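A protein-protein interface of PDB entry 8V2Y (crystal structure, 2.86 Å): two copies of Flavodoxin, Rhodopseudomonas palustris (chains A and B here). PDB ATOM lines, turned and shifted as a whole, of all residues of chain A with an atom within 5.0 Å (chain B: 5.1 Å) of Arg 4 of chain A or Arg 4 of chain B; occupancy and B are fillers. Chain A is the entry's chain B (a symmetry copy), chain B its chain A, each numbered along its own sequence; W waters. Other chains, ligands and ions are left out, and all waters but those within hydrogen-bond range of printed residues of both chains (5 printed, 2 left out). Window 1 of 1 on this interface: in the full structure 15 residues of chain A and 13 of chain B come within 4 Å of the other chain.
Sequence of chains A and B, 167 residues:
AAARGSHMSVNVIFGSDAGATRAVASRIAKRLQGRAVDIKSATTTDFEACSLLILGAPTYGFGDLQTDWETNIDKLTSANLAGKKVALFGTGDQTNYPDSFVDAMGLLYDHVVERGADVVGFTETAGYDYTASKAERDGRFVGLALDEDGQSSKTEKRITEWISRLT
OG of Ser 6 of chain A lies within hydrogen-bond range of NE of Arg 4 of chain B (2.5 Å).
NH2 of Arg 4 of chain A sits at hydrogen-bond distance from OG of Ser 6 of chain B (3.0 Å).
The backbone NH (N) of Ser 9 of chain B lies within hydrogen-bond range of the backbone carbonyl oxygen (O) of Ala 2 of chain A (2.8 Å).
The backbone NH of Ser 9 of chain A is in hydrogen-bond range of the backbone carbonyl oxygen of Ala 2 of chain B (3.0 Å).
The guanidinium group (NH2) of Arg 4 of chain B sits at hydrogen-bond distance from the side-chain amide oxygen (OD1) of Asn 11 of chain A.
The side-chain amide oxygen (OD1) of Asn 11 of chain B lies within hydrogen-bond range of the guanidinium group (NH2) of Arg 4 of chain A.
NH2 of Arg 4 of chain B lies within hydrogen-bond range of O of Val 10 of chain A (3.0 Å).
N of Arg 4 of chain B is in hydrogen-bond range of O of His 7 of chain A (3.1 Å).
The backbone carbonyl oxygen (O) of Met 8 of chain B sits at hydrogen-bond distance from the guanidinium group (NE) of Arg 4 of chain A (3.0 Å).
The guanidinium group (NE) of Arg 4 of chain B lies within hydrogen-bond range of the backbone carbonyl oxygen (O) of Met 8 of chain A (3.1 Å).
The backbone carbonyl oxygen of Val 10 of chain B lies within hydrogen-bond range of the guanidinium group of Arg 4 of chain A, at 3.1 Å.
NH1 of Arg 4 of chain B sits at hydrogen-bond distance from O of Ala 49 of chain A.
The backbone carbonyl oxygen (O) of His 7 of chain B is in hydrogen-bond range of the backbone NH (N) of Arg 4 of chain A, 3.0 Å away.
The side-chain amide nitrogen (ND2) of Asn 11 of chain A is in hydrogen-bond range of the backbone carbonyl oxygen (O) of Ala 49 of chain A, 3.4 Å away.
OG of Ser 6 of chain A lies within hydrogen-bond range of O of Met 8 of chain A, 2.8 Å away.
OD1 of Asn 11 of chain A is in hydrogen-bond range of NH1 of Arg 35 of chain A (3.1 Å).
O of Met 8 of chain B lies within hydrogen-bond range of OG of Ser 6 of chain B (2.7 Å).
O of Val 10 of chain A lies within hydrogen-bond range of N of Arg 35 of chain A (3.0 Å).
The backbone carbonyl oxygen of Val 10 of chain B lies within hydrogen-bond range of the backbone NH of Arg 35 of chain B.
Among the printed residues, pairs that only touch across the chains: Met 8 of chain A with Ala 2 of chain B (3.3 Å), Arg 35 of chain A with Arg 4 of chain B (3.4 Å), Ser 9 of chain A with Arg 4 of chain B (3.5 Å), Ala 49 of chain A with Ala 49 of chain B (3.5 Å), Arg 4 of chain A with Ser 9 of chain B (3.7 Å), Arg 4 of chain A with Arg 4 of chain B (3.7 Å), Ala 3 of chain A with His 7 of chain B (3.7 Å), Ala 2 of chain A with Met 8 of chain B (3.7 Å), Ala 3 of chain A with Met 8 of chain B (3.8 Å), Met 8 of chain A with Ala 3 of chain B (3.8 Å), Arg 4 of chain A with Arg 35 of chain B (3.8 Å), Arg 4 of chain A with Ala 49 of chain B (3.8 Å) and Ser 9 of chain A with Ala 3 of chain B (3.998 Å).
Of chain B, only Arg 4 (3.7 Å), Ser 6 (3.0 Å), His 7 (3.0 Å), Met 8 (3.0 Å), Ser 9 (3.7 Å), Val 10 (3.1 Å), Asn 11 (2.9 Å), Arg 35 (3.8 Å) and Ala 49 (3.8 Å) come within 4 Å of Arg 4 of chain A.
Arg 4 of chain B touches nine residues of chain A.
Of the printed residues of chain B, Asn 11 of chain A touches Arg 4.
Of the printed residues of chain B, Ser 9 of chain A touches Ala 2 (3.0 Å), Ala 3 (3.998 Å) and Arg 4 (3.5 Å).
Printed residues of chain B within 4 Å of Arg 35 of chain A: Arg 4 (3.4 Å).
Printed residues of chain B within 4 Å of Ala 49 of chain A: Arg 4 and Ala 49.
Gly 5 of chain A touches none of the printed residues of chain B.
Cys 50 of chain A touches none of the printed residues of chain B.
The nearest residue of chain A that does not touch Arg 4 of chain B is Cys 50 of chain A (4.8 Å).
The nearest printed residue of chain A that does not touch Ala 3 of chain B is His 7 of chain A (4.03 Å).
Printed residues of chain B that touch a printed residue of chain A: Ala 2, Ala 3, Arg 4, Ser 6, His 7, Met 8, Ser 9, Val 10, Asn 11, Arg 35 and Ala 49.
Of the 13 printed residues of chain A, 11 touch a printed residue of chain B.
Hydrophobic or aromatic side chains of chain A that line the printed part of chain B: Ala 3, Met 8 and Ala 49.
Along chain A the printed residues that touch a printed residue of chain B span positions 2 to 49.
Among the printed residues, 26 pairs touch across the chains.
Among the printed residues, no Asp or Glu carboxylate lies within 4 Å of a Lys or Arg side-chain nitrogen of the other chain.
Ala 3 of chain A touches His 7 of chain B, but with the chains exchanged His 7 of chain A does not touch Ala 3 of chain B (4.03 Å).
Arg 4 of chain B touches its own counterpart, Arg 4 of chain A.
Arg 4 of chain A touches Ser 6 of chain B, and with the chains exchanged Ser 6 of chain A touches Arg 4 of chain B.
Arg 4 of chain A touches Ser 9 of chain B, and with the chains exchanged Ser 9 of chain A touches Arg 4 of chain B.
Of the 26 pairs that touch across the chains among the printed residues, 24 have their exchanged pair printed and touching as well.
Water W1 bridges the backbone carbonyl oxygen (O) of Ser 6 of chain A (2.6 Å) and the backbone carbonyl oxygen (O) of Ser 6 of chain B (3.0 Å).
Water W3 bridges the guanidinium group of Arg 4 of chain B (2.7 Å) and the backbone carbonyl oxygen of Ala 49 of chain A (3.4 Å).
Water W4 lies within hydrogen-bond range of N of Ala 2 of chain A (2.8 Å) and O of Ser 9 of chain B (3.4 Å).
Water W2 lies within hydrogen-bond range of O of Ala 49 of chain B, ND2 of Asn 11 of chain B and NH1 of Arg 4 of chain A.
Water W5 lies within hydrogen-bond range of OG of Ser 9 of chain A and O of Ala 3 of chain B.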
ATOM      1  N   ALA A   2       2.825  19.645  11.184  1.00  0.00           N
ATOM      2  CA  ALA A   2       1.732  20.120  10.349  1.00  0.00           C
ATOM      3  C   ALA A   2       1.164  21.413  10.920  1.00  0.00           C
ATOM      4  O   ALA A   2       1.004  21.549  12.138  1.00  0.00           O
ATOM      5  CB  ALA A   2       0.627  19.065  10.244  1.00  0.00           C
ATOM      6  N   ALA A   3       0.867  22.363  10.035  1.00  0.00           N
ATOM      7  CA  ALA A   3       0.246  23.606  10.463  1.00  0.00           C
ATOM      8  C   ALA A   3      -1.201  23.363  10.882  1.00  0.00           C
ATOM      9  O   ALA A   3      -1.855  22.426  10.416  1.00  0.00           O
ATOM     10  CB  ALA A   3       0.307  24.644   9.343  1.00  0.00           C
ATOM     11  N   ARG A   4      -1.698  24.215  11.784  1.00  0.00           N
ATOM     12  CA  ARG A   4      -3.090  24.101  12.215  1.00  0.00           C
ATOM     13  C   ARG A   4      -4.065  24.400  11.086  1.00  0.00           C
ATOM     14  O   ARG A   4      -5.193  23.895  11.099  1.00  0.00           O
ATOM     15  CB  ARG A   4      -3.368  25.024  13.396  1.00  0.00           C
ATOM     16  CG  ARG A   4      -2.443  24.811  14.569  1.00  0.00           C
ATOM     17  CD  ARG A   4      -2.934  25.555  15.793  1.00  0.00           C
ATOM     18  NE  ARG A   4      -2.036  25.368  16.927  1.00  0.00           N
ATOM     19  CZ  ARG A   4      -2.222  24.480  17.892  1.00  0.00           C
ATOM     20  NH1 ARG A   4      -3.287  23.694  17.913  1.00  0.00           N
ATOM     21  NH2 ARG A   4      -1.320  24.380  18.864  1.00  0.00           N
ATOM     22  N   GLY A   5      -3.670  25.226  10.122  1.00  0.00           N
ATOM     23  CA  GLY A   5      -4.516  25.543   8.990  1.00  0.00           C
ATOM     24  C   GLY A   5      -5.114  26.928   9.038  1.00  0.00           C
ATOM     25  O   GLY A   5      -5.620  27.402   8.012  1.00  0.00           O
ATOM     26  N   SER A   6      -5.084  27.589  10.190  1.00  0.00           N
ATOM     27  CA  SER A   6      -5.581  28.952  10.279  1.00  0.00           C
ATOM     28  C   SER A   6      -4.929  29.638  11.465  1.00  0.00           C
ATOM     29  O   SER A   6      -4.625  29.007  12.480  1.00  0.00           O
ATOM     30  CB  SER A   6      -7.107  28.976  10.423  1.00  0.00           C
ATOM     31  OG  SER A   6      -7.513  28.422  11.663  1.00  0.00           O
ATOM     32  N   HIS A   7      -4.726  30.944  11.320  1.00  0.00           N
ATOM     33  CA  HIS A   7      -4.159  31.733  12.406  1.00  0.00           C
ATOM     34  C   HIS A   7      -5.156  31.905  13.546  1.00  0.00           C
ATOM     35  O   HIS A   7      -4.834  31.658  14.715  1.00  0.00           O
ATOM     36  CB  HIS A   7      -3.676  33.079  11.856  1.00  0.00           C
ATOM     37  CG  HIS A   7      -3.505  34.148  12.889  1.00  0.00           C
ATOM     38  ND1 HIS A   7      -2.873  33.935  14.095  1.00  0.00           N
ATOM     39  CD2 HIS A   7      -3.871  35.453  12.882  1.00  0.00           C
ATOM     40  CE1 HIS A   7      -2.866  35.058  14.791  1.00  0.00           C
ATOM     41  NE2 HIS A   7      -3.465  35.995  14.077  1.00  0.00           N
ATOM     42  N   MET A   8      -6.374  32.322  13.219  1.00  0.00           N
ATOM     43  CA  MET A   8      -7.430  32.502  14.203  1.00  0.00           C
ATOM     44  C   MET A   8      -8.125  31.177  14.500  1.00  0.00           C
ATOM     45  O   MET A   8      -8.180  30.274  13.659  1.00  0.00           O
ATOM     46  CB  MET A   8      -8.462  33.497  13.696  1.00  0.00           C
ATOM     47  CG  MET A   8      -7.946  34.902  13.551  1.00  0.00           C
ATOM     48  SD  MET A   8      -7.395  35.437  15.183  1.00  0.00           S
ATOM     49  CE  MET A   8      -8.919  35.521  16.105  1.00  0.00           C
ATOM     50  N   SER A   9      -8.699  31.086  15.701  1.00  0.00           N
ATOM     51  CA  SER A   9      -9.415  29.884  16.135  1.00  0.00           C
ATOM     52  C   SER A   9     -10.871  29.902  15.663  1.00  0.00           C
ATOM     53  O   SER A   9     -11.816  30.041  16.443  1.00  0.00           O
ATOM     54  CB  SER A   9      -9.316  29.781  17.649  1.00  0.00           C
ATOM     55  OG  SER A   9      -9.562  28.459  18.088  1.00  0.00           O
ATOM     56  N   VAL A  10     -11.045  29.739  14.351  1.00  0.00           N
ATOM     57  CA  VAL A  10     -12.365  29.688  13.734  1.00  0.00           C
ATOM     58  C   VAL A  10     -12.450  28.445  12.861  1.00  0.00           C
ATOM     59  O   VAL A  10     -11.615  28.247  11.972  1.00  0.00           O
ATOM     60  CB  VAL A  10     -12.672  30.946  12.895  1.00  0.00           C
ATOM     61  CG1 VAL A  10     -14.099  30.890  12.365  1.00  0.00           C
ATOM     62  CG2 VAL A  10     -12.458  32.213  13.713  1.00  0.00           C
ATOM     63  N   ASN A  11     -13.467  27.624  13.098  1.00  0.00           N
ATOM     64  CA  ASN A  11     -13.720  26.432  12.300  1.00  0.00           C
ATOM     65  C   ASN A  11     -15.056  26.604  11.597  1.00  0.00           C
ATOM     66  O   ASN A  11     -16.089  26.778  12.255  1.00  0.00           O
ATOM     67  CB  ASN A  11     -13.726  25.171  13.166  1.00  0.00           C
ATOM     68  CG  ASN A  11     -12.337  24.624  13.408  1.00  0.00           C
ATOM     69  OD1 ASN A  11     -11.363  25.085  12.814  1.00  0.00           O
ATOM     70  ND2 ASN A  11     -12.240  23.620  14.270  1.00  0.00           N
ATOM     71  N   ARG A  35     -10.597  27.954   9.192  1.00  0.00           N
ATOM     72  CA  ARG A  35     -10.551  26.738   8.392  1.00  0.00           C
ATOM     73  C   ARG A  35     -11.927  26.436   7.817  1.00  0.00           C
ATOM     74  O   ARG A  35     -12.944  26.581   8.503  1.00  0.00           O
ATOM     75  CB  ARG A  35     -10.075  25.544   9.223  1.00  0.00           C
ATOM     76  CG  ARG A  35      -8.690  25.693   9.816  1.00  0.00           C
ATOM     77  CD  ARG A  35      -8.380  24.537  10.751  1.00  0.00           C
ATOM     78  NE  ARG A  35      -8.577  23.244  10.105  1.00  0.00           N
ATOM     79  CZ  ARG A  35      -9.436  22.323  10.519  1.00  0.00           C
ATOM     80  NH1 ARG A  35     -10.195  22.514  11.585  1.00  0.00           N
ATOM     81  NH2 ARG A  35      -9.534  21.179   9.848  1.00  0.00           N
ATOM     82  N   ALA A  49     -12.542  22.227  18.666  1.00  0.00           N
ATOM     83  CA  ALA A  49     -11.248  22.906  18.733  1.00  0.00           C
ATOM     84  C   ALA A  49     -11.302  24.271  18.047  1.00  0.00           C
ATOM     85  O   ALA A  49     -10.587  24.545  17.082  1.00  0.00           O
ATOM     86  CB  ALA A  49     -10.161  22.029  18.126  1.00  0.00           C
ATOM     87  N   CYS A  50     -12.176  25.132  18.562  1.00  0.00           N
ATOM     88  CA  CYS A  50     -12.283  26.496  18.061  1.00  0.00           C
ATOM     89  C   CYS A  50     -13.053  27.337  19.066  1.00  0.00           C
ATOM     90  O   CYS A  50     -13.965  26.849  19.740  1.00  0.00           O
ATOM     91  CB  CYS A  50     -12.966  26.549  16.691  1.00  0.00           C
ATOM     92  SG  CYS A  50     -14.628  25.864  16.672  1.00  0.00           S
ATOM     93  N   ALA B   2     -10.588  34.762  19.225  1.00  0.00           N
ATOM     94  CA  ALA B   2      -9.320  34.445  19.873  1.00  0.00           C
ATOM     95  C   ALA B   2      -8.400  33.684  18.923  1.00  0.00           C
ATOM     96  O   ALA B   2      -8.861  32.868  18.117  1.00  0.00           O
ATOM     97  CB  ALA B   2      -9.555  33.625  21.144  1.00  0.00           C
ATOM     98  N   ALA B   3      -7.104  33.969  19.006  1.00  0.00           N
ATOM     99  CA  ALA B   3      -6.135  33.266  18.177  1.00  0.00           C
ATOM    100  C   ALA B   3      -6.001  31.805  18.597  1.00  0.00           C
ATOM    101  O   ALA B   3      -6.278  31.431  19.740  1.00  0.00           O
ATOM    102  CB  ALA B   3      -4.773  33.960  18.257  1.00  0.00           C
ATOM    103  N   ARG B   4      -5.582  30.966  17.645  1.00  0.00           N
ATOM    104  CA  ARG B   4      -5.377  29.557  17.968  1.00  0.00           C
ATOM    105  C   ARG B   4      -4.277  29.394  19.004  1.00  0.00           C
ATOM    106  O   ARG B   4      -4.313  28.452  19.803  1.00  0.00           O
ATOM    107  CB  ARG B   4      -5.067  28.758  16.706  1.00  0.00           C
ATOM    108  CG  ARG B   4      -6.320  28.268  16.010  1.00  0.00           C
ATOM    109  CD  ARG B   4      -6.025  27.356  14.843  1.00  0.00           C
ATOM    110  NE  ARG B   4      -7.123  27.344  13.881  1.00  0.00           N
ATOM    111  CZ  ARG B   4      -8.269  26.697  14.055  1.00  0.00           C
ATOM    112  NH1 ARG B   4      -8.497  25.970  15.137  1.00  0.00           N
ATOM    113  NH2 ARG B   4      -9.205  26.773  13.114  1.00  0.00           N
ATOM    114  N   GLY B   5      -3.313  30.312  19.023  1.00  0.00           N
ATOM    115  CA  GLY B   5      -2.257  30.341  20.009  1.00  0.00           C
ATOM    116  C   GLY B   5      -0.910  29.888  19.496  1.00  0.00           C
ATOM    117  O   GLY B   5       0.109  30.175  20.137  1.00  0.00           O
ATOM    118  N   SER B   6      -0.875  29.179  18.372  1.00  0.00           N
ATOM    119  CA  SER B   6       0.380  28.771  17.758  1.00  0.00           C
ATOM    120  C   SER B   6       0.110  28.405  16.306  1.00  0.00           C
ATOM    121  O   SER B   6      -0.998  27.998  15.955  1.00  0.00           O
ATOM    122  CB  SER B   6       1.026  27.609  18.520  1.00  0.00           C
ATOM    123  OG  SER B   6       0.713  26.356  17.942  1.00  0.00           O
ATOM    124  N   HIS B   7       1.129  28.569  15.463  1.00  0.00           N
ATOM    125  CA  HIS B   7       0.976  28.242  14.049  1.00  0.00           C
ATOM    126  C   HIS B   7       0.913  26.733  13.817  1.00  0.00           C
ATOM    127  O   HIS B   7      -0.001  26.239  13.147  1.00  0.00           O
ATOM    128  CB  HIS B   7       2.119  28.857  13.244  1.00  0.00           C
ATOM    129  CG  HIS B   7       2.080  28.520  11.786  1.00  0.00           C
ATOM    130  ND1 HIS B   7       1.230  29.146  10.898  1.00  0.00           N
ATOM    131  CD2 HIS B   7       2.786  27.620  11.060  1.00  0.00           C
ATOM    132  CE1 HIS B   7       1.415  28.648   9.689  1.00  0.00           C
ATOM    133  NE2 HIS B   7       2.353  27.719   9.759  1.00  0.00           N
ATOM    134  N   MET B   8       1.881  25.988  14.348  1.00  0.00           N
ATOM    135  CA  MET B   8       1.916  24.540  14.169  1.00  0.00           C
ATOM    136  C   MET B   8       0.984  23.824  15.138  1.00  0.00           C
ATOM    137  O   MET B   8       0.680  24.315  16.228  1.00  0.00           O
ATOM    138  CB  MET B   8       3.340  24.013  14.337  1.00  0.00           C
ATOM    139  CG  MET B   8       4.312  24.580  13.322  1.00  0.00           C
ATOM    140  SD  MET B   8       3.731  24.369  11.627  1.00  0.00           S
ATOM    141  CE  MET B   8       5.084  23.443  10.913  1.00  0.00           C
ATOM    142  N   SER B   9       0.533  22.637  14.724  1.00  0.00           N
ATOM    143  CA  SER B   9      -0.397  21.827  15.513  1.00  0.00           C
ATOM    144  C   SER B   9       0.381  21.004  16.542  1.00  0.00           C
ATOM    145  O   SER B   9       0.487  19.777  16.471  1.00  0.00           O
ATOM    146  CB  SER B   9      -1.231  20.936  14.603  1.00  0.00           C
ATOM    147  OG  SER B   9      -2.373  20.446  15.283  1.00  0.00           O
ATOM    148  N   VAL B  10       0.929  21.717  17.524  1.00  0.00           N
ATOM    149  CA  VAL B  10       1.679  21.120  18.621  1.00  0.00           C
ATOM    150  C   VAL B  10       1.112  21.651  19.931  1.00  0.00           C
ATOM    151  O   VAL B  10       1.026  22.868  20.128  1.00  0.00           O
ATOM    152  CB  VAL B  10       3.185  21.429  18.519  1.00  0.00           C
ATOM    153  CG1 VAL B  10       3.941  20.778  19.666  1.00  0.00           C
ATOM    154  CG2 VAL B  10       3.733  20.958  17.180  1.00  0.00           C
ATOM    155  N   ASN B  11       0.720  20.744  20.820  1.00  0.00           N
ATOM    156  CA  ASN B  11       0.214  21.102  22.138  1.00  0.00           C
ATOM    157  C   ASN B  11       1.137  20.522  23.197  1.00  0.00           C
ATOM    158  O   ASN B  11       1.342  19.305  23.245  1.00  0.00           O
ATOM    159  CB  ASN B  11      -1.215  20.602  22.337  1.00  0.00           C
ATOM    160  CG  ASN B  11      -2.229  21.460  21.621  1.00  0.00           C
ATOM    161  OD1 ASN B  11      -1.874  22.424  20.940  1.00  0.00           O
ATOM    162  ND2 ASN B  11      -3.501  21.122  21.775  1.00  0.00           N
ATOM    163  N   GLY B  34       4.433  25.708  19.044  1.00  0.00           N
ATOM    164  CA  GLY B  34       3.275  25.118  19.670  1.00  0.00           C
ATOM    165  C   GLY B  34       2.770  25.943  20.844  1.00  0.00           C
ATOM    166  O   GLY B  34       3.312  26.985  21.197  1.00  0.00           O
ATOM    167  N   ARG B  35       1.694  25.442  21.441  1.00  0.00           N
ATOM    168  CA  ARG B  35       1.073  26.057  22.604  1.00  0.00           C
ATOM    169  C   ARG B  35       1.542  25.369  23.873  1.00  0.00           C
ATOM    170  O   ARG B  35       1.652  24.142  23.921  1.00  0.00           O
ATOM    171  CB  ARG B  35      -0.450  25.975  22.533  1.00  0.00           C
ATOM    172  CG  ARG B  35      -1.088  26.983  21.627  1.00  0.00           C
ATOM    173  CD  ARG B  35      -2.591  26.822  21.640  1.00  0.00           C
ATOM    174  NE  ARG B  35      -3.028  25.537  22.178  1.00  0.00           N
ATOM    175  CZ  ARG B  35      -3.984  25.390  23.086  1.00  0.00           C
ATOM    176  NH1 ARG B  35      -4.620  26.432  23.598  1.00  0.00           N
ATOM    177  NH2 ARG B  35      -4.323  24.164  23.478  1.00  0.00           N
ATOM    178  N   ALA B  49      -6.735  17.713  19.844  1.00  0.00           N
ATOM    179  CA  ALA B  49      -6.688  18.636  18.709  1.00  0.00           C
ATOM    180  C   ALA B  49      -5.256  19.070  18.396  1.00  0.00           C
ATOM    181  O   ALA B  49      -4.922  20.254  18.414  1.00  0.00           O
ATOM    182  CB  ALA B  49      -7.570  19.846  18.986  1.00  0.00           C
HETATM  183  O   HOH W   1      -2.241  29.057  13.416  1.00  0.00           O
HETATM  184  O   HOH W   2      -5.546  22.627  20.119  1.00  0.00           O
HETATM  185  O   HOH W   3      -7.302  25.512  17.481  1.00  0.00           O
HETATM  186  O   HOH W   4       2.496  18.855  13.835  1.00  0.00           O
HETATM  187  O   HOH W   5      -8.438  29.417  20.753  1.00  0.00           O
